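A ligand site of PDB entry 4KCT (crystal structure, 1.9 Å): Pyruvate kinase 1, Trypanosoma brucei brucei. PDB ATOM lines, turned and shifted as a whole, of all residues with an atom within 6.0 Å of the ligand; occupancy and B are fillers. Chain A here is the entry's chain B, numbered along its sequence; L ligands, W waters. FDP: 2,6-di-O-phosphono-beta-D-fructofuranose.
The side-chain hydroxyl (OG) of Ser 401 lies within hydrogen-bond range of the backbone NH (N) of Ser 406 (3.5 Å). N of Arg 405 sits at hydrogen-bond distance from OG of Ser 401. OG of Ser 401 is in hydrogen-bond range of N of Gly 404, 2.9 Å away. N of Leu 400 lies within hydrogen-bond range of O of Val 480, 3.2 Å away. The side-chain amino group (NZ) of Lys 454 is in hydrogen-bond range of the backbone carbonyl oxygen (O) of Lys 452, at 3.0 Å. The side-chain amide oxygen of Asn 402 lies within hydrogen-bond range of the side-chain hydroxyl of Thr 424 (2.8 Å). NE of Arg 457 lies within salt-bridge range of OD2 of Asp 451 (2.8 Å). N of Arg 405 sits at hydrogen-bond distance from OG1 of Thr 403, at 3.1 Å.
Water W8 bridges O5P of the ligand and ND2 of Asn 402. Water W6 lies within hydrogen-bond range of an oxygen (O6P) of the ligand, the guanidinium group of Arg 405 and the backbone carbonyl oxygen of Gly 488. Water W1 bridges an oxygen (O6P) of the ligand and the backbone carbonyl oxygen of Gly 488. Water W2 lies within hydrogen-bond range of an oxygen (O3P) of the ligand, the side-chain amino group (NZ) of Lys 454 and the side-chain amino group (NZ) of Lys 487. Water W7 bridges O1 of the ligand (3.3 Å) and N of Gly 488 (3.4 Å).
Residues that only touch the ligand: His 481 (3.4 Å), Lys 487 (3.4 Å), Pro 490 (3.5 Å), Arg 405 (3.6 Å) and Val 486 (3.7 Å). Hydrophobic or aromatic side chains within 4 Å of the ligand: Leu 400, His 481, Ala 482 and Pro 490. Within 4 Å of the ligand: Leu 400, Ser 401, Asn 402, Thr 403, Arg 405, Ser 406, Lys 454, Arg 457, His 481, Ala 482, Val 486, Lys 487, Gly 488, Tyr 489 and Pro 490. The nearest printed residue that does not touch the ligand is Gly 404 (4.4 Å).
The side-chain hydroxyl (OG) of Ser 401 sits at hydrogen-bond distance from an oxygen (O4P) of the ligand (2.6 Å). O of Leu 400 lies within hydrogen-bond range of O4 of the ligand. O4P of the ligand is in hydrogen-bond range of N of Ser 406 (2.9 Å). O4P of the ligand is in hydrogen-bond range of OG of Ser 406 (2.7 Å). NZ of Lys 454 is in salt-bridge range of O1P of the ligand (2.7 Å). The backbone NH (N) of Asn 402 sits at hydrogen-bond distance from an oxygen (O5P) of the ligand. The side-chain amide nitrogen (ND2) of Asn 402 sits at hydrogen-bond distance from an oxygen (O2P) of the ligand (2.9 Å). An oxygen (O2P) of the ligand lies within salt-bridge range of the guanidinium group (NH1) of Arg 457. O1 of the ligand is in hydrogen-bond range of N of Gly 488 (2.9 Å). The backbone NH (N) of Thr 403 is in hydrogen-bond range of an oxygen (O5P) of the ligand. OG1 of Thr 403 is in hydrogen-bond range of O6P of the ligand (3.0 Å). N of Ala 482 is in hydrogen-bond range of O3 of the ligand (3.0 Å). N of Tyr 489 lies within hydrogen-bond range of O5 of the ligand, 3.4 Å away.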
ATOM      1  N   VAL A 399      -4.258  22.696   4.004  1.00  0.00           N
ATOM      2  CA  VAL A 399      -5.276  23.662   4.420  1.00  0.00           C
ATOM      3  C   VAL A 399      -6.560  23.436   3.619  1.00  0.00           C
ATOM      4  O   VAL A 399      -6.499  23.131   2.421  1.00  0.00           O
ATOM      5  CB  VAL A 399      -4.790  25.145   4.250  1.00  0.00           C
ATOM      6  CG1 VAL A 399      -4.407  25.444   2.791  1.00  0.00           C
ATOM      7  CG2 VAL A 399      -5.836  26.147   4.790  1.00  0.00           C
ATOM      8  N   LEU A 400      -7.704  23.469   4.294  1.00  0.00           N
ATOM      9  CA  LEU A 400      -9.019  23.478   3.593  1.00  0.00           C
ATOM     10  C   LEU A 400      -9.414  24.916   3.285  1.00  0.00           C
ATOM     11  O   LEU A 400      -9.436  25.768   4.175  1.00  0.00           O
ATOM     12  CB  LEU A 400     -10.102  22.820   4.459  1.00  0.00           C
ATOM     13  CG  LEU A 400     -10.194  21.288   4.378  1.00  0.00           C
ATOM     14  CD1 LEU A 400      -8.804  20.662   4.490  1.00  0.00           C
ATOM     15  CD2 LEU A 400     -11.124  20.735   5.457  1.00  0.00           C
ATOM     16  N   SER A 401      -9.579  25.229   1.995  1.00  0.00           N
ATOM     17  CA  SER A 401      -9.963  26.585   1.630  1.00  0.00           C
ATOM     18  C   SER A 401     -10.906  26.528   0.465  1.00  0.00           C
ATOM     19  O   SER A 401     -10.631  25.881  -0.523  1.00  0.00           O
ATOM     20  CB  SER A 401      -8.728  27.435   1.252  1.00  0.00           C
ATOM     21  OG  SER A 401      -9.128  28.786   1.029  1.00  0.00           O
ATOM     22  N   ASN A 402     -12.052  27.179   0.606  1.00  0.00           N
ATOM     23  CA  ASN A 402     -13.043  27.205  -0.461  1.00  0.00           C
ATOM     24  C   ASN A 402     -12.910  28.428  -1.350  1.00  0.00           C
ATOM     25  O   ASN A 402     -13.028  28.324  -2.585  1.00  0.00           O
ATOM     26  CB  ASN A 402     -14.451  27.105   0.129  1.00  0.00           C
ATOM     27  CG  ASN A 402     -14.611  25.886   1.024  1.00  0.00           C
ATOM     28  OD1 ASN A 402     -14.263  24.768   0.625  1.00  0.00           O
ATOM     29  ND2 ASN A 402     -14.989  26.113   2.273  1.00  0.00           N
ATOM     30  N   THR A 403     -12.552  29.560  -0.753  1.00  0.00           N
ATOM     31  CA  THR A 403     -12.406  30.812  -1.526  1.00  0.00           C
ATOM     32  C   THR A 403     -10.951  31.006  -1.960  1.00  0.00           C
ATOM     33  O   THR A 403     -10.650  31.898  -2.727  1.00  0.00           O
ATOM     34  CB  THR A 403     -12.818  32.042  -0.695  1.00  0.00           C
ATOM     35  OG1 THR A 403     -11.905  32.211   0.409  1.00  0.00           O
ATOM     36  CG2 THR A 403     -14.258  31.901  -0.160  1.00  0.00           C
ATOM     37  N   GLY A 404     -10.040  30.289  -1.323  1.00  0.00           N
ATOM     38  CA  GLY A 404      -8.603  30.559  -1.507  1.00  0.00           C
ATOM     39  C   GLY A 404      -7.993  31.344  -0.360  1.00  0.00           C
ATOM     40  O   GLY A 404      -6.775  31.372  -0.204  1.00  0.00           O
ATOM     41  N   ARG A 405      -8.823  32.019   0.427  1.00  0.00           N
ATOM     42  CA  ARG A 405      -8.336  32.990   1.390  1.00  0.00           C
ATOM     43  C   ARG A 405      -7.344  32.369   2.428  1.00  0.00           C
ATOM     44  O   ARG A 405      -6.286  32.950   2.693  1.00  0.00           O
ATOM     45  CB  ARG A 405      -9.501  33.644   2.125  1.00  0.00           C
ATOM     46  CG  ARG A 405      -9.068  34.797   3.005  1.00  0.00           C
ATOM     47  CD  ARG A 405     -10.205  35.389   3.822  1.00  0.00           C
ATOM     48  NE  ARG A 405      -9.652  36.202   4.912  1.00  0.00           N
ATOM     49  CZ  ARG A 405      -9.817  35.963   6.210  1.00  0.00           C
ATOM     50  NH1 ARG A 405      -9.156  36.698   7.102  1.00  0.00           N
ATOM     51  NH2 ARG A 405     -10.715  35.072   6.623  1.00  0.00           N
ATOM     52  N   SER A 406      -7.712  31.239   3.014  1.00  0.00           N
ATOM     53  CA  SER A 406      -6.857  30.585   4.009  1.00  0.00           C
ATOM     54  C   SER A 406      -5.567  30.099   3.405  1.00  0.00           C
ATOM     55  O   SER A 406      -4.533  30.061   4.075  1.00  0.00           O
ATOM     56  CB  SER A 406      -7.575  29.404   4.679  1.00  0.00           C
ATOM     57  OG  SER A 406      -8.796  29.816   5.284  1.00  0.00           O
ATOM     58  N   ALA A 407      -5.612  29.658   2.148  1.00  0.00           N
ATOM     59  CA  ALA A 407      -4.359  29.216   1.501  1.00  0.00           C
ATOM     60  C   ALA A 407      -3.402  30.392   1.302  1.00  0.00           C
ATOM     61  O   ALA A 407      -2.183  30.260   1.517  1.00  0.00           O
ATOM     62  CB  ALA A 407      -4.634  28.505   0.184  1.00  0.00           C
ATOM     63  N   THR A 424     -13.178  23.153  -2.586  1.00  0.00           N
ATOM     64  CA  THR A 424     -14.430  22.684  -3.179  1.00  0.00           C
ATOM     65  C   THR A 424     -14.780  23.436  -4.465  1.00  0.00           C
ATOM     66  O   THR A 424     -15.866  23.237  -5.024  1.00  0.00           O
ATOM     67  CB  THR A 424     -15.582  22.866  -2.189  1.00  0.00           C
ATOM     68  OG1 THR A 424     -15.581  24.221  -1.727  1.00  0.00           O
ATOM     69  CG2 THR A 424     -15.401  21.940  -0.990  1.00  0.00           C
ATOM     70  N   ARG A 425     -13.894  24.316  -4.925  1.00  0.00           N
ATOM     71  CA  ARG A 425     -14.130  25.071  -6.154  1.00  0.00           C
ATOM     72  C   ARG A 425     -12.993  24.939  -7.153  1.00  0.00           C
ATOM     73  O   ARG A 425     -11.853  25.269  -6.859  1.00  0.00           O
ATOM     74  CB  ARG A 425     -14.352  26.549  -5.848  1.00  0.00           C
ATOM     75  CG  ARG A 425     -15.606  26.832  -5.047  1.00  0.00           C
ATOM     76  CD  ARG A 425     -15.753  28.316  -4.771  1.00  0.00           C
ATOM     77  NE  ARG A 425     -16.412  28.528  -3.493  1.00  0.00           N
ATOM     78  CZ  ARG A 425     -16.441  29.679  -2.840  1.00  0.00           C
ATOM     79  NH1 ARG A 425     -15.942  30.786  -3.378  1.00  0.00           N
ATOM     80  NH2 ARG A 425     -17.012  29.727  -1.650  1.00  0.00           N
ATOM     81  N   ASP A 451     -19.208  16.868   3.948  1.00  0.00           N
ATOM     82  CA  ASP A 451     -17.960  16.774   4.716  1.00  0.00           C
ATOM     83  C   ASP A 451     -17.838  17.812   5.846  1.00  0.00           C
ATOM     84  O   ASP A 451     -16.768  18.388   6.067  1.00  0.00           O
ATOM     85  CB  ASP A 451     -16.743  16.873   3.792  1.00  0.00           C
ATOM     86  CG  ASP A 451     -15.473  16.397   4.456  1.00  0.00           C
ATOM     87  OD1 ASP A 451     -15.553  15.426   5.263  1.00  0.00           O
ATOM     88  OD2 ASP A 451     -14.415  17.045   4.273  1.00  0.00           O
ATOM     89  N   LYS A 452     -18.897  17.932   6.660  1.00  0.00           N
ATOM     90  CA  LYS A 452     -18.935  18.908   7.768  1.00  0.00           C
ATOM     91  C   LYS A 452     -17.806  18.695   8.762  1.00  0.00           C
ATOM     92  O   LYS A 452     -17.295  19.665   9.340  1.00  0.00           O
ATOM     93  CB  LYS A 452     -20.278  18.842   8.514  1.00  0.00           C
ATOM     94  CG  LYS A 452     -21.402  19.621   7.860  1.00  0.00           C
ATOM     95  CD  LYS A 452     -22.618  19.675   8.780  1.00  0.00           C
ATOM     96  CE  LYS A 452     -23.122  21.103   8.954  1.00  0.00           C
ATOM     97  NZ  LYS A 452     -24.545  21.256   8.508  1.00  0.00           N
ATOM     98  N   LYS A 454     -14.857  17.541   8.079  1.00  0.00           N
ATOM     99  CA  LYS A 454     -13.553  17.745   7.393  1.00  0.00           C
ATOM    100  C   LYS A 454     -12.791  16.469   7.038  1.00  0.00           C
ATOM    101  O   LYS A 454     -11.761  16.526   6.379  1.00  0.00           O
ATOM    102  CB  LYS A 454     -12.602  18.700   8.176  1.00  0.00           C
ATOM    103  CG  LYS A 454     -13.260  19.598   9.207  1.00  0.00           C
ATOM    104  CD  LYS A 454     -13.985  20.723   8.524  1.00  0.00           C
ATOM    105  CE  LYS A 454     -14.634  21.652   9.536  1.00  0.00           C
ATOM    106  NZ  LYS A 454     -15.837  22.244   8.892  1.00  0.00           N
ATOM    107  N   ARG A 457     -12.112  15.523   3.239  1.00  0.00           N
ATOM    108  CA  ARG A 457     -11.177  16.434   2.633  1.00  0.00           C
ATOM    109  C   ARG A 457      -9.762  16.266   3.159  1.00  0.00           C
ATOM    110  O   ARG A 457      -8.810  16.345   2.386  1.00  0.00           O
ATOM    111  CB  ARG A 457     -11.656  17.892   2.763  1.00  0.00           C
ATOM    112  CG  ARG A 457     -12.730  18.210   1.741  1.00  0.00           C
ATOM    113  CD  ARG A 457     -13.361  19.559   2.006  1.00  0.00           C
ATOM    114  NE  ARG A 457     -14.052  19.607   3.288  1.00  0.00           N
ATOM    115  CZ  ARG A 457     -14.419  20.733   3.879  1.00  0.00           C
ATOM    116  NH1 ARG A 457     -14.039  21.901   3.356  1.00  0.00           N
ATOM    117  NH2 ARG A 457     -15.138  20.714   5.004  1.00  0.00           N
ATOM    118  N   VAL A 480      -4.542  22.575   8.719  1.00  0.00           N
ATOM    119  CA  VAL A 480      -5.250  23.771   9.155  1.00  0.00           C
ATOM    120  C   VAL A 480      -6.677  23.737   8.584  1.00  0.00           C
ATOM    121  O   VAL A 480      -6.861  23.621   7.359  1.00  0.00           O
ATOM    122  CB  VAL A 480      -4.543  25.042   8.655  1.00  0.00           C
ATOM    123  CG1 VAL A 480      -5.371  26.304   8.987  1.00  0.00           C
ATOM    124  CG2 VAL A 480      -3.110  25.133   9.252  1.00  0.00           C
ATOM    125  N   HIS A 481      -7.666  23.850   9.458  1.00  0.00           N
ATOM    126  CA  HIS A 481      -9.075  24.052   9.039  1.00  0.00           C
ATOM    127  C   HIS A 481      -9.862  24.466  10.247  1.00  0.00           C
ATOM    128  O   HIS A 481      -9.282  24.866  11.259  1.00  0.00           O
ATOM    129  CB  HIS A 481      -9.664  22.790   8.380  1.00  0.00           C
ATOM    130  CG  HIS A 481      -9.497  21.516   9.199  1.00  0.00           C
ATOM    131  ND1 HIS A 481     -10.281  21.230  10.286  1.00  0.00           N
ATOM    132  CD2 HIS A 481      -8.686  20.400   8.995  1.00  0.00           C
ATOM    133  CE1 HIS A 481      -9.924  20.011  10.773  1.00  0.00           C
ATOM    134  NE2 HIS A 481      -8.978  19.489   9.975  1.00  0.00           N
ATOM    135  N   ALA A 482     -11.207  24.383  10.196  1.00  0.00           N
ATOM    136  CA  ALA A 482     -11.986  24.751  11.402  1.00  0.00           C
ATOM    137  C   ALA A 482     -12.297  23.515  12.253  1.00  0.00           C
ATOM    138  O   ALA A 482     -12.149  22.376  11.779  1.00  0.00           O
ATOM    139  CB  ALA A 482     -13.267  25.474  11.031  1.00  0.00           C
ATOM    140  N   ASP A 483     -12.581  23.739  13.533  1.00  0.00           N
ATOM    141  CA  ASP A 483     -13.065  22.659  14.377  1.00  0.00           C
ATOM    142  C   ASP A 483     -14.513  22.366  14.011  1.00  0.00           C
ATOM    143  O   ASP A 483     -14.996  22.824  12.952  1.00  0.00           O
ATOM    144  CB  ASP A 483     -12.900  22.991  15.884  1.00  0.00           C
ATOM    145  CG  ASP A 483     -13.786  24.163  16.325  1.00  0.00           C
ATOM    146  OD1 ASP A 483     -14.773  24.488  15.619  1.00  0.00           O
ATOM    147  OD2 ASP A 483     -13.469  24.790  17.367  1.00  0.00           O
ATOM    148  N   VAL A 486     -16.960  25.905  14.329  1.00  0.00           N
ATOM    149  CA  VAL A 486     -16.667  27.245  13.785  1.00  0.00           C
ATOM    150  C   VAL A 486     -16.843  27.284  12.257  1.00  0.00           C
ATOM    151  O   VAL A 486     -16.437  26.360  11.556  1.00  0.00           O
ATOM    152  CB  VAL A 486     -15.258  27.714  14.215  1.00  0.00           C
ATOM    153  CG1 VAL A 486     -14.791  28.894  13.351  1.00  0.00           C
ATOM    154  CG2 VAL A 486     -15.268  28.148  15.676  1.00  0.00           C
ATOM    155  N   LYS A 487     -17.546  28.309  11.761  1.00  0.00           N
ATOM    156  CA  LYS A 487     -17.757  28.490  10.313  1.00  0.00           C
ATOM    157  C   LYS A 487     -17.160  29.816   9.838  1.00  0.00           C
ATOM    158  O   LYS A 487     -17.216  30.821  10.543  1.00  0.00           O
ATOM    159  CB  LYS A 487     -19.249  28.505   9.958  1.00  0.00           C
ATOM    160  CG  LYS A 487     -20.024  27.295  10.438  1.00  0.00           C
ATOM    161  CD  LYS A 487     -19.450  25.989   9.892  1.00  0.00           C
ATOM    162  CE  LYS A 487     -20.051  24.813  10.629  1.00  0.00           C
ATOM    163  NZ  LYS A 487     -19.395  23.519  10.303  1.00  0.00           N
ATOM    164  N   GLY A 488     -16.655  29.828   8.597  1.00  0.00           N
ATOM    165  CA  GLY A 488     -16.280  31.074   7.951  1.00  0.00           C
ATOM    166  C   GLY A 488     -14.767  31.254   7.822  1.00  0.00           C
ATOM    167  O   GLY A 488     -14.304  32.082   7.074  1.00  0.00           O
ATOM    168  N   TYR A 489     -14.004  30.465   8.575  1.00  0.00           N
ATOM    169  CA  TYR A 489     -12.550  30.635   8.664  1.00  0.00           C
ATOM    170  C   TYR A 489     -11.954  29.453   9.444  1.00  0.00           C
ATOM    171  O   TYR A 489     -12.681  28.748  10.162  1.00  0.00           O
ATOM    172  CB  TYR A 489     -12.181  31.969   9.337  1.00  0.00           C
ATOM    173  CG  TYR A 489     -12.623  32.092  10.784  1.00  0.00           C
ATOM    174  CD1 TYR A 489     -13.915  32.539  11.124  1.00  0.00           C
ATOM    175  CD2 TYR A 489     -11.766  31.708  11.831  1.00  0.00           C
ATOM    176  CE1 TYR A 489     -14.328  32.615  12.459  1.00  0.00           C
ATOM    177  CE2 TYR A 489     -12.167  31.820  13.165  1.00  0.00           C
ATOM    178  CZ  TYR A 489     -13.444  32.263  13.470  1.00  0.00           C
ATOM    179  OH  TYR A 489     -13.858  32.300  14.794  1.00  0.00           O
ATOM    180  N   PRO A 490     -10.641  29.210   9.304  1.00  0.00           N
ATOM    181  CA  PRO A 490     -10.010  28.118  10.076  1.00  0.00           C
ATOM    182  C   PRO A 490      -9.592  28.614  11.473  1.00  0.00           C
ATOM    183  O   PRO A 490      -8.941  29.658  11.599  1.00  0.00           O
ATOM    184  CB  PRO A 490      -8.763  27.776   9.248  1.00  0.00           C
ATOM    185  CG  PRO A 490      -8.362  29.122   8.656  1.00  0.00           C
ATOM    186  CD  PRO A 490      -9.705  29.811   8.328  1.00  0.00           C
HETATM  187  P1  FDP L   1     -15.572  24.393   5.749  1.00  0.00           P
HETATM  188  O1P FDP L   1     -14.955  23.251   6.525  1.00  0.00           O
HETATM  189  O2P FDP L   1     -15.584  24.117   4.267  1.00  0.00           O
HETATM  190  O3P FDP L   1     -16.877  24.929   6.313  1.00  0.00           O
HETATM  191  O1  FDP L   1     -16.223  27.174   7.611  1.00  0.00           O
HETATM  192  C1  FDP L   1     -15.108  26.443   8.109  1.00  0.00           C
HETATM  193  C2  FDP L   1     -14.050  26.360   7.012  1.00  0.00           C
HETATM  194  O2  FDP L   1     -14.515  25.636   5.848  1.00  0.00           O
HETATM  195  C3  FDP L   1     -12.731  25.774   7.500  1.00  0.00           C
HETATM  196  O3  FDP L   1     -12.809  24.353   7.653  1.00  0.00           O
HETATM  197  C4  FDP L   1     -11.811  26.164   6.356  1.00  0.00           C
HETATM  198  O4  FDP L   1     -10.421  26.043   6.686  1.00  0.00           O
HETATM  199  C5  FDP L   1     -12.237  27.595   6.120  1.00  0.00           C
HETATM  200  O5  FDP L   1     -13.641  27.681   6.582  1.00  0.00           O
HETATM  201  C6  FDP L   1     -12.130  27.970   4.646  1.00  0.00           C
HETATM  202  O6  FDP L   1     -12.240  29.386   4.539  1.00  0.00           O
HETATM  203  P2  FDP L   1     -11.816  30.101   3.142  1.00  0.00           P
HETATM  204  O4P FDP L   1     -10.306  29.873   3.026  1.00  0.00           O
HETATM  205  O5P FDP L   1     -12.637  29.386   2.124  1.00  0.00           O
HETATM  206  O6P FDP L   1     -12.179  31.553   3.350  1.00  0.00           O
HETATM  207  O   HOH W   1     -14.745  31.485   3.818  1.00  0.00           O
HETATM  208  O   HOH W   2     -18.421  22.949   7.389  1.00  0.00           O
HETATM  209  O   HOH W   3     -15.620  29.067   5.229  1.00  0.00           O
HETATM  210  O   HOH W   4     -17.555  23.296   2.736  1.00  0.00           O
HETATM  211  O   HOH W   5     -18.931  25.865   5.010  1.00  0.00           O
HETATM  212  O   HOH W   6     -11.923  32.740   5.614  1.00  0.00           O
HETATM  213  O   HOH W   7     -18.435  28.876   5.828  1.00  0.00           O
HETATM  214  O   HOH W   8     -15.030  29.079   2.702  1.00  0.00           O
